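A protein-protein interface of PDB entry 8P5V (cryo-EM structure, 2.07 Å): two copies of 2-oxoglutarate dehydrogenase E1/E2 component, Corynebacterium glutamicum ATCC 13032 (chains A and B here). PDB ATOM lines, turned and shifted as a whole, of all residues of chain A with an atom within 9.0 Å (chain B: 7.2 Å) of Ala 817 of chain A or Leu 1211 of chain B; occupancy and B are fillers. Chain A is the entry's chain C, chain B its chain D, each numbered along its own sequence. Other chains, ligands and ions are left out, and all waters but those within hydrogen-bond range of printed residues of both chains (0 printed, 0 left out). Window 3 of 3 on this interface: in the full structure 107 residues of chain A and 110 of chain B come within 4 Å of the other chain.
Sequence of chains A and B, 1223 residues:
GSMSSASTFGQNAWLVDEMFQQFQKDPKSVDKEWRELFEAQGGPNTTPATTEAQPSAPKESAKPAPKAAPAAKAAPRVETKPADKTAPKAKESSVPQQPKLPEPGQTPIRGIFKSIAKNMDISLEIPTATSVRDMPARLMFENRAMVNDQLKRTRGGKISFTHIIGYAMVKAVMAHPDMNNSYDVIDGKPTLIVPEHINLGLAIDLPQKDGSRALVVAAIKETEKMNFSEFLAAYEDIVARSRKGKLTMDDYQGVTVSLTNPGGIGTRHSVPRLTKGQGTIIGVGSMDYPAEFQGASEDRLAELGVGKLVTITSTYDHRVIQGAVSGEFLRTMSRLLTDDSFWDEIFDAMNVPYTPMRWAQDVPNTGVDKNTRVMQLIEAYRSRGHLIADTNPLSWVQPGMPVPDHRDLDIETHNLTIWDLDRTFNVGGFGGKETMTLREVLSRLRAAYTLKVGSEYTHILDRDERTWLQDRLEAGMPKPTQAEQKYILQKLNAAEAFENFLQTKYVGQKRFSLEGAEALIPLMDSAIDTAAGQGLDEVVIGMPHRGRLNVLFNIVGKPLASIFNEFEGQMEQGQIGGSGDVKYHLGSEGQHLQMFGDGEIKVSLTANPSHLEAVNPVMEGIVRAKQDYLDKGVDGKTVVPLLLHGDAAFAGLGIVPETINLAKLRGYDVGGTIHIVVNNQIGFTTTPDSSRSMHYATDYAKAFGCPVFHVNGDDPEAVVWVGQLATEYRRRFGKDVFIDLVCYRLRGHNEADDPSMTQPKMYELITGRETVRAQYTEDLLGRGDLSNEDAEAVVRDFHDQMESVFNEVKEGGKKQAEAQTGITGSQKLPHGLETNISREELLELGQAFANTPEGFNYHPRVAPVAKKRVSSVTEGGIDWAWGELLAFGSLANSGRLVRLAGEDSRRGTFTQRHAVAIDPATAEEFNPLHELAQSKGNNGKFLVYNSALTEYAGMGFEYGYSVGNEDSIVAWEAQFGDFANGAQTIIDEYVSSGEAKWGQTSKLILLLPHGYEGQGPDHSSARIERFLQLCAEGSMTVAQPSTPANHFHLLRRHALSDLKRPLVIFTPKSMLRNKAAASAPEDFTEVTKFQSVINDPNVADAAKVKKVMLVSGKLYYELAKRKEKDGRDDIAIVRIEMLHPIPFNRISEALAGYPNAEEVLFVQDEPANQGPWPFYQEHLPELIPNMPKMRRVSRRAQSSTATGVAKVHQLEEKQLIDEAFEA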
ATOM      1  N   GLY A 569      -2.942 -17.862  32.677  1.00  0.00           N
ATOM      2  CA  GLY A 569      -2.508 -18.853  31.704  1.00  0.00           C
ATOM      3  C   GLY A 569      -2.004 -18.219  30.409  1.00  0.00           C
ATOM      4  O   GLY A 569      -1.287 -18.864  29.647  1.00  0.00           O
ATOM      5  N   GLN A 570      -2.391 -16.960  30.166  1.00  0.00           N
ATOM      6  CA  GLN A 570      -1.985 -16.235  28.973  1.00  0.00           C
ATOM      7  C   GLN A 570      -0.557 -15.729  29.154  1.00  0.00           C
ATOM      8  O   GLN A 570      -0.323 -14.764  29.879  1.00  0.00           O
ATOM      9  CB  GLN A 570      -2.946 -15.079  28.685  1.00  0.00           C
ATOM     10  CG  GLN A 570      -4.273 -15.518  28.080  1.00  0.00           C
ATOM     11  CD  GLN A 570      -5.141 -16.310  29.029  1.00  0.00           C
ATOM     12  OE1 GLN A 570      -4.863 -16.422  30.224  1.00  0.00           O
ATOM     13  NE2 GLN A 570      -6.224 -16.851  28.491  1.00  0.00           N
ATOM     14  N   LYS A 814     -10.787 -15.590  28.113  1.00  0.00           N
ATOM     15  CA  LYS A 814      -9.709 -16.529  28.375  1.00  0.00           C
ATOM     16  C   LYS A 814      -9.578 -17.484  27.189  1.00  0.00           C
ATOM     17  O   LYS A 814     -10.386 -18.398  27.037  1.00  0.00           O
ATOM     18  CB  LYS A 814      -9.974 -17.299  29.673  1.00  0.00           C
ATOM     19  N   LYS A 815      -8.559 -17.250  26.352  1.00  0.00           N
ATOM     20  CA  LYS A 815      -8.271 -18.105  25.212  1.00  0.00           C
ATOM     21  C   LYS A 815      -7.879 -19.500  25.698  1.00  0.00           C
ATOM     22  O   LYS A 815      -7.201 -19.640  26.715  1.00  0.00           O
ATOM     23  CB  LYS A 815      -7.152 -17.499  24.358  1.00  0.00           C
ATOM     24  N   GLN A 816      -8.318 -20.521  24.949  1.00  0.00           N
ATOM     25  CA  GLN A 816      -8.050 -21.911  25.286  1.00  0.00           C
ATOM     26  C   GLN A 816      -6.611 -22.258  24.911  1.00  0.00           C
ATOM     27  O   GLN A 816      -5.930 -21.481  24.241  1.00  0.00           O
ATOM     28  CB  GLN A 816      -9.045 -22.839  24.581  1.00  0.00           C
ATOM     29  CG  GLN A 816      -8.917 -22.859  23.063  1.00  0.00           C
ATOM     30  CD  GLN A 816      -9.941 -23.753  22.404  1.00  0.00           C
ATOM     31  OE1 GLN A 816     -10.761 -24.387  23.064  1.00  0.00           O
ATOM     32  NE2 GLN A 816      -9.898 -23.811  21.082  1.00  0.00           N
ATOM     33  N   ALA A 817      -6.165 -23.442  25.351  1.00  0.00           N
ATOM     34  CA  ALA A 817      -4.822 -23.922  25.070  1.00  0.00           C
ATOM     35  C   ALA A 817      -4.694 -24.253  23.585  1.00  0.00           C
ATOM     36  O   ALA A 817      -5.650 -24.718  22.965  1.00  0.00           O
ATOM     37  CB  ALA A 817      -4.515 -25.124  25.928  1.00  0.00           C
ATOM     38  N   GLU A 818      -3.499 -24.007  23.030  1.00  0.00           N
ATOM     39  CA  GLU A 818      -3.222 -24.266  21.627  1.00  0.00           C
ATOM     40  C   GLU A 818      -1.868 -24.960  21.510  1.00  0.00           C
ATOM     41  O   GLU A 818      -1.017 -24.817  22.386  1.00  0.00           O
ATOM     42  CB  GLU A 818      -3.286 -22.960  20.826  1.00  0.00           C
ATOM     43  CG  GLU A 818      -1.967 -22.202  20.705  1.00  0.00           C
ATOM     44  CD  GLU A 818      -1.311 -21.771  22.007  1.00  0.00           C
ATOM     45  OE1 GLU A 818      -0.175 -21.261  21.948  1.00  0.00           O
ATOM     46  OE2 GLU A 818      -1.936 -21.938  23.072  1.00  0.00           O
ATOM     47  N   ALA A 819      -1.685 -25.706  20.415  1.00  0.00           N
ATOM     48  CA  ALA A 819      -0.432 -26.390  20.144  1.00  0.00           C
ATOM     49  C   ALA A 819       0.612 -25.376  19.682  1.00  0.00           C
ATOM     50  O   ALA A 819       0.302 -24.470  18.910  1.00  0.00           O
ATOM     51  CB  ALA A 819      -0.647 -27.468  19.111  1.00  0.00           C
ATOM     52  N   GLN A 820       1.849 -25.545  20.167  1.00  0.00           N
ATOM     53  CA  GLN A 820       2.954 -24.664  19.823  1.00  0.00           C
ATOM     54  C   GLN A 820       3.708 -25.275  18.646  1.00  0.00           C
ATOM     55  O   GLN A 820       4.068 -26.450  18.683  1.00  0.00           O
ATOM     56  CB  GLN A 820       3.853 -24.451  21.044  1.00  0.00           C
ATOM     57  CG  GLN A 820       3.087 -23.983  22.274  1.00  0.00           C
ATOM     58  CD  GLN A 820       3.965 -23.821  23.491  1.00  0.00           C
ATOM     59  OE1 GLN A 820       3.940 -24.637  24.408  1.00  0.00           O
ATOM     60  NE2 GLN A 820       4.749 -22.758  23.509  1.00  0.00           N
ATOM     61  N   ARG B1195       5.513 -36.626  22.352  1.00  0.00           N
ATOM     62  CA  ARG B1195       5.515 -35.206  22.043  1.00  0.00           C
ATOM     63  C   ARG B1195       6.492 -34.926  20.902  1.00  0.00           C
ATOM     64  O   ARG B1195       7.387 -35.725  20.642  1.00  0.00           O
ATOM     65  CB  ARG B1195       5.894 -34.401  23.289  1.00  0.00           C
ATOM     66  CG  ARG B1195       4.917 -34.545  24.444  1.00  0.00           C
ATOM     67  CD  ARG B1195       5.289 -33.644  25.605  1.00  0.00           C
ATOM     68  NE  ARG B1195       4.198 -33.448  26.551  1.00  0.00           N
ATOM     69  CZ  ARG B1195       3.631 -34.398  27.291  1.00  0.00           C
ATOM     70  NH1 ARG B1195       4.098 -35.634  27.277  1.00  0.00           N
ATOM     71  NH2 ARG B1195       2.597 -34.106  28.058  1.00  0.00           N
ATOM     72  N   VAL B1205       3.979 -23.603  29.733  1.00  0.00           N
ATOM     73  CA  VAL B1205       2.558 -23.391  29.958  1.00  0.00           C
ATOM     74  C   VAL B1205       1.933 -24.704  30.421  1.00  0.00           C
ATOM     75  O   VAL B1205       2.056 -25.713  29.737  1.00  0.00           O
ATOM     76  CB  VAL B1205       1.865 -22.866  28.684  1.00  0.00           C
ATOM     77  CG1 VAL B1205       0.426 -22.455  28.955  1.00  0.00           C
ATOM     78  CG2 VAL B1205       2.643 -21.726  28.049  1.00  0.00           C
ATOM     79  N   ALA B1206       1.229 -24.665  31.558  1.00  0.00           N
ATOM     80  CA  ALA B1206       0.686 -25.860  32.185  1.00  0.00           C
ATOM     81  C   ALA B1206      -0.535 -26.378  31.428  1.00  0.00           C
ATOM     82  O   ALA B1206      -0.766 -27.584  31.388  1.00  0.00           O
ATOM     83  CB  ALA B1206       0.342 -25.570  33.625  1.00  0.00           C
ATOM     84  N   LYS B1207      -1.329 -25.467  30.851  1.00  0.00           N
ATOM     85  CA  LYS B1207      -2.558 -25.847  30.171  1.00  0.00           C
ATOM     86  C   LYS B1207      -2.224 -26.519  28.841  1.00  0.00           C
ATOM     87  O   LYS B1207      -2.993 -27.344  28.355  1.00  0.00           O
ATOM     88  CB  LYS B1207      -3.456 -24.620  29.971  1.00  0.00           C
ATOM     89  CG  LYS B1207      -4.951 -24.887  29.818  1.00  0.00           C
ATOM     90  CD  LYS B1207      -5.621 -25.596  30.991  1.00  0.00           C
ATOM     91  CE  LYS B1207      -5.419 -24.908  32.325  1.00  0.00           C
ATOM     92  NZ  LYS B1207      -5.966 -23.530  32.328  1.00  0.00           N
ATOM     93  N   VAL B1208      -1.075 -26.158  28.258  1.00  0.00           N
ATOM     94  CA  VAL B1208      -0.606 -26.797  27.039  1.00  0.00           C
ATOM     95  C   VAL B1208      -0.265 -28.256  27.342  1.00  0.00           C
ATOM     96  O   VAL B1208      -0.544 -29.142  26.528  1.00  0.00           O
ATOM     97  CB  VAL B1208       0.598 -26.050  26.435  1.00  0.00           C
ATOM     98  CG1 VAL B1208       1.259 -26.836  25.311  1.00  0.00           C
ATOM     99  CG2 VAL B1208       0.214 -24.654  25.968  1.00  0.00           C
ATOM    100  N   HIS B1209       0.345 -28.500  28.512  1.00  0.00           N
ATOM    101  CA  HIS B1209       0.753 -29.838  28.913  1.00  0.00           C
ATOM    102  C   HIS B1209      -0.438 -30.792  28.910  1.00  0.00           C
ATOM    103  O   HIS B1209      -0.319 -31.914  28.431  1.00  0.00           O
ATOM    104  CB  HIS B1209       1.479 -29.817  30.261  1.00  0.00           C
ATOM    105  CG  HIS B1209       1.531 -31.148  30.946  1.00  0.00           C
ATOM    106  ND1 HIS B1209       0.506 -31.355  31.837  1.00  0.00           N
ATOM    107  CD2 HIS B1209       2.254 -32.270  30.954  1.00  0.00           C
ATOM    108  CE1 HIS B1209       0.613 -32.558  32.379  1.00  0.00           C
ATOM    109  NE2 HIS B1209       1.663 -33.126  31.854  1.00  0.00           N
ATOM    110  N   GLN B1210      -1.574 -30.342  29.455  1.00  0.00           N
ATOM    111  CA  GLN B1210      -2.763 -31.176  29.525  1.00  0.00           C
ATOM    112  C   GLN B1210      -3.263 -31.479  28.119  1.00  0.00           C
ATOM    113  O   GLN B1210      -3.732 -32.587  27.863  1.00  0.00           O
ATOM    114  CB  GLN B1210      -3.870 -30.508  30.344  1.00  0.00           C
ATOM    115  CG  GLN B1210      -3.410 -29.981  31.690  1.00  0.00           C
ATOM    116  CD  GLN B1210      -3.143 -31.037  32.738  1.00  0.00           C
ATOM    117  OE1 GLN B1210      -3.616 -32.171  32.670  1.00  0.00           O
ATOM    118  NE2 GLN B1210      -2.390 -30.649  33.750  1.00  0.00           N
ATOM    119  N   LEU B1211      -3.158 -30.498  27.212  1.00  0.00           N
ATOM    120  CA  LEU B1211      -3.632 -30.659  25.846  1.00  0.00           C
ATOM    121  C   LEU B1211      -2.794 -31.720  25.135  1.00  0.00           C
ATOM    122  O   LEU B1211      -3.345 -32.589  24.461  1.00  0.00           O
ATOM    123  CB  LEU B1211      -3.560 -29.313  25.117  1.00  0.00           C
ATOM    124  CG  LEU B1211      -4.075 -29.312  23.677  1.00  0.00           C
ATOM    125  CD1 LEU B1211      -5.595 -29.339  23.644  1.00  0.00           C
ATOM    126  CD2 LEU B1211      -3.547 -28.108  22.910  1.00  0.00           C
ATOM    127  N   GLU B1212      -1.465 -31.635  25.285  1.00  0.00           N
ATOM    128  CA  GLU B1212      -0.573 -32.538  24.578  1.00  0.00           C
ATOM    129  C   GLU B1212      -0.681 -33.943  25.156  1.00  0.00           C
ATOM    130  O   GLU B1212      -0.577 -34.915  24.416  1.00  0.00           O
ATOM    131  CB  GLU B1212       0.867 -32.035  24.531  1.00  0.00           C
ATOM    132  CG  GLU B1212       1.486 -31.565  25.815  1.00  0.00           C
ATOM    133  CD  GLU B1212       2.769 -30.768  25.600  1.00  0.00           C
ATOM    134  OE1 GLU B1212       2.785 -29.884  24.713  1.00  0.00           O
ATOM    135  OE2 GLU B1212       3.734 -31.000  26.345  1.00  0.00           O
ATOM    136  N   GLU B1213      -0.904 -34.041  26.469  1.00  0.00           N
ATOM    137  CA  GLU B1213      -1.083 -35.327  27.129  1.00  0.00           C
ATOM    138  C   GLU B1213      -2.315 -36.030  26.558  1.00  0.00           C
ATOM    139  O   GLU B1213      -2.250 -37.214  26.231  1.00  0.00           O
ATOM    140  CB  GLU B1213      -1.202 -35.142  28.643  1.00  0.00           C
ATOM    141  CG  GLU B1213      -1.436 -36.422  29.432  1.00  0.00           C
ATOM    142  CD  GLU B1213      -0.204 -37.176  29.904  1.00  0.00           C
ATOM    143  OE1 GLU B1213      -0.377 -38.200  30.604  1.00  0.00           O
ATOM    144  OE2 GLU B1213       0.920 -36.740  29.580  1.00  0.00           O
ATOM    145  N   LYS B1214      -3.428 -35.294  26.436  1.00  0.00           N
ATOM    146  CA  LYS B1214      -4.651 -35.850  25.886  1.00  0.00           C
ATOM    147  C   LYS B1214      -4.417 -36.268  24.435  1.00  0.00           C
ATOM    148  O   LYS B1214      -4.902 -37.311  24.005  1.00  0.00           O
ATOM    149  CB  LYS B1214      -5.798 -34.840  25.984  1.00  0.00           C
ATOM    150  CG  LYS B1214      -7.134 -35.336  25.441  1.00  0.00           C
ATOM    151  CD  LYS B1214      -8.231 -34.295  25.458  1.00  0.00           C
ATOM    152  CE  LYS B1214      -9.454 -34.704  24.661  1.00  0.00           C
ATOM    153  NZ  LYS B1214     -10.098 -35.922  25.213  1.00  0.00           N
ATOM    154  N   GLN B1215      -3.678 -35.438  23.691  1.00  0.00           N
ATOM    155  CA  GLN B1215      -3.383 -35.704  22.293  1.00  0.00           C
ATOM    156  C   GLN B1215      -2.521 -36.959  22.176  1.00  0.00           C
ATOM    157  O   GLN B1215      -2.711 -37.760  21.266  1.00  0.00           O
ATOM    158  CB  GLN B1215      -2.677 -34.500  21.669  1.00  0.00           C
ATOM    159  CG  GLN B1215      -2.290 -34.691  20.210  1.00  0.00           C
ATOM    160  CD  GLN B1215      -1.483 -33.533  19.670  1.00  0.00           C
ATOM    161  OE1 GLN B1215      -1.236 -32.542  20.356  1.00  0.00           O
ATOM    162  NE2 GLN B1215      -1.059 -33.654  18.423  1.00  0.00           N
ATOM    163  N   LEU B1216      -1.573 -37.108  23.106  1.00  0.00           N
ATOM    164  CA  LEU B1216      -0.632 -38.215  23.103  1.00  0.00           C
ATOM    165  C   LEU B1216      -1.378 -39.537  23.268  1.00  0.00           C
ATOM    166  O   LEU B1216      -1.128 -40.484  22.527  1.00  0.00           O
ATOM    167  CB  LEU B1216       0.384 -37.983  24.226  1.00  0.00           C
ATOM    168  CG  LEU B1216       1.613 -38.887  24.232  1.00  0.00           C
ATOM    169  CD1 LEU B1216       2.775 -38.197  24.929  1.00  0.00           C
ATOM    170  CD2 LEU B1216       1.319 -40.214  24.914  1.00  0.00           C
ATOM    171  N   ILE B1217      -2.307 -39.590  24.232  1.00  0.00           N
ATOM    172  CA  ILE B1217      -3.037 -40.813  24.530  1.00  0.00           C
ATOM    173  C   ILE B1217      -3.984 -41.135  23.375  1.00  0.00           C
ATOM    174  O   ILE B1217      -4.139 -42.298  23.015  1.00  0.00           O
ATOM    175  CB  ILE B1217      -3.774 -40.716  25.883  1.00  0.00           C
ATOM    176  CG1 ILE B1217      -2.805 -40.385  27.029  1.00  0.00           C
ATOM    177  CG2 ILE B1217      -4.565 -41.991  26.164  1.00  0.00           C
ATOM    178  CD1 ILE B1217      -3.449 -40.256  28.385  1.00  0.00           C
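Among the printed residues, pairs that only touch across the chains: Gln 820 of chain A with Val 1208 of chain B (3.6 Å), Ala 817 of chain A with Lys 1207 of chain B (3.6 Å), Glu 818 of chain A with Val 1208 of chain B (3.8 Å), Glu 818 of chain A with Leu 1211 of chain B (3.8 Å), Ala 819 of chain A with Leu 1211 of chain B (3.9 Å) and Ala 817 of chain A with Leu 1211 of chain B (3.99 Å).
Printed residues of chain A within 4 Å of Leu 1211 of chain B: Ala 817 (3.99 Å), Glu 818 (3.8 Å) and Ala 819 (3.9 Å).
Printed residues of chain B within 4 Å of Gln 820 of chain A: Val 1208.
Printed residues of chain B within 4 Å of Ala 819 of chain A: Leu 1211 (3.9 Å).
Of the printed residues of chain A, Lys 1207 of chain B touches Ala 817 (3.6 Å).
Of the printed residues of chain B, Glu 818 of chain A touches Val 1208 (3.8 Å) and Leu 1211 (3.8 Å).
Of the printed residues of chain A, Val 1208 of chain B touches Glu 818 and Gln 820.
Ala 1206 of chain B touches none of the printed residues of chain A.
Lys 1214 of chain B touches none of the printed residues of chain A.
The nearest printed residue of chain B that does not touch Ala 817 of chain A is Val 1208 of chain B (4.3 Å).
The nearest printed residue of chain A that does not touch Leu 1211 of chain B is Gln 820 of chain A (6.6 Å).
The nearest printed residue of chain B that does not touch Ala 819 of chain A is Gln 1215 of chain B (5.3 Å).
Hydrophobic or aromatic side chains of chain A within 4 Å of the printed part of chain B: Ala 817.
Along chain A the printed residues that touch a printed residue of chain B span positions 817 to 820.
Hydrophobic or aromatic side chains of chain B within 4 Å of the printed part of chain A: Val 1208 and Leu 1211.
Among the printed residues, no Asp or Glu carboxylate lies within 4 Å of a Lys or Arg side-chain nitrogen of the other chain.
No position is printed for both chains.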
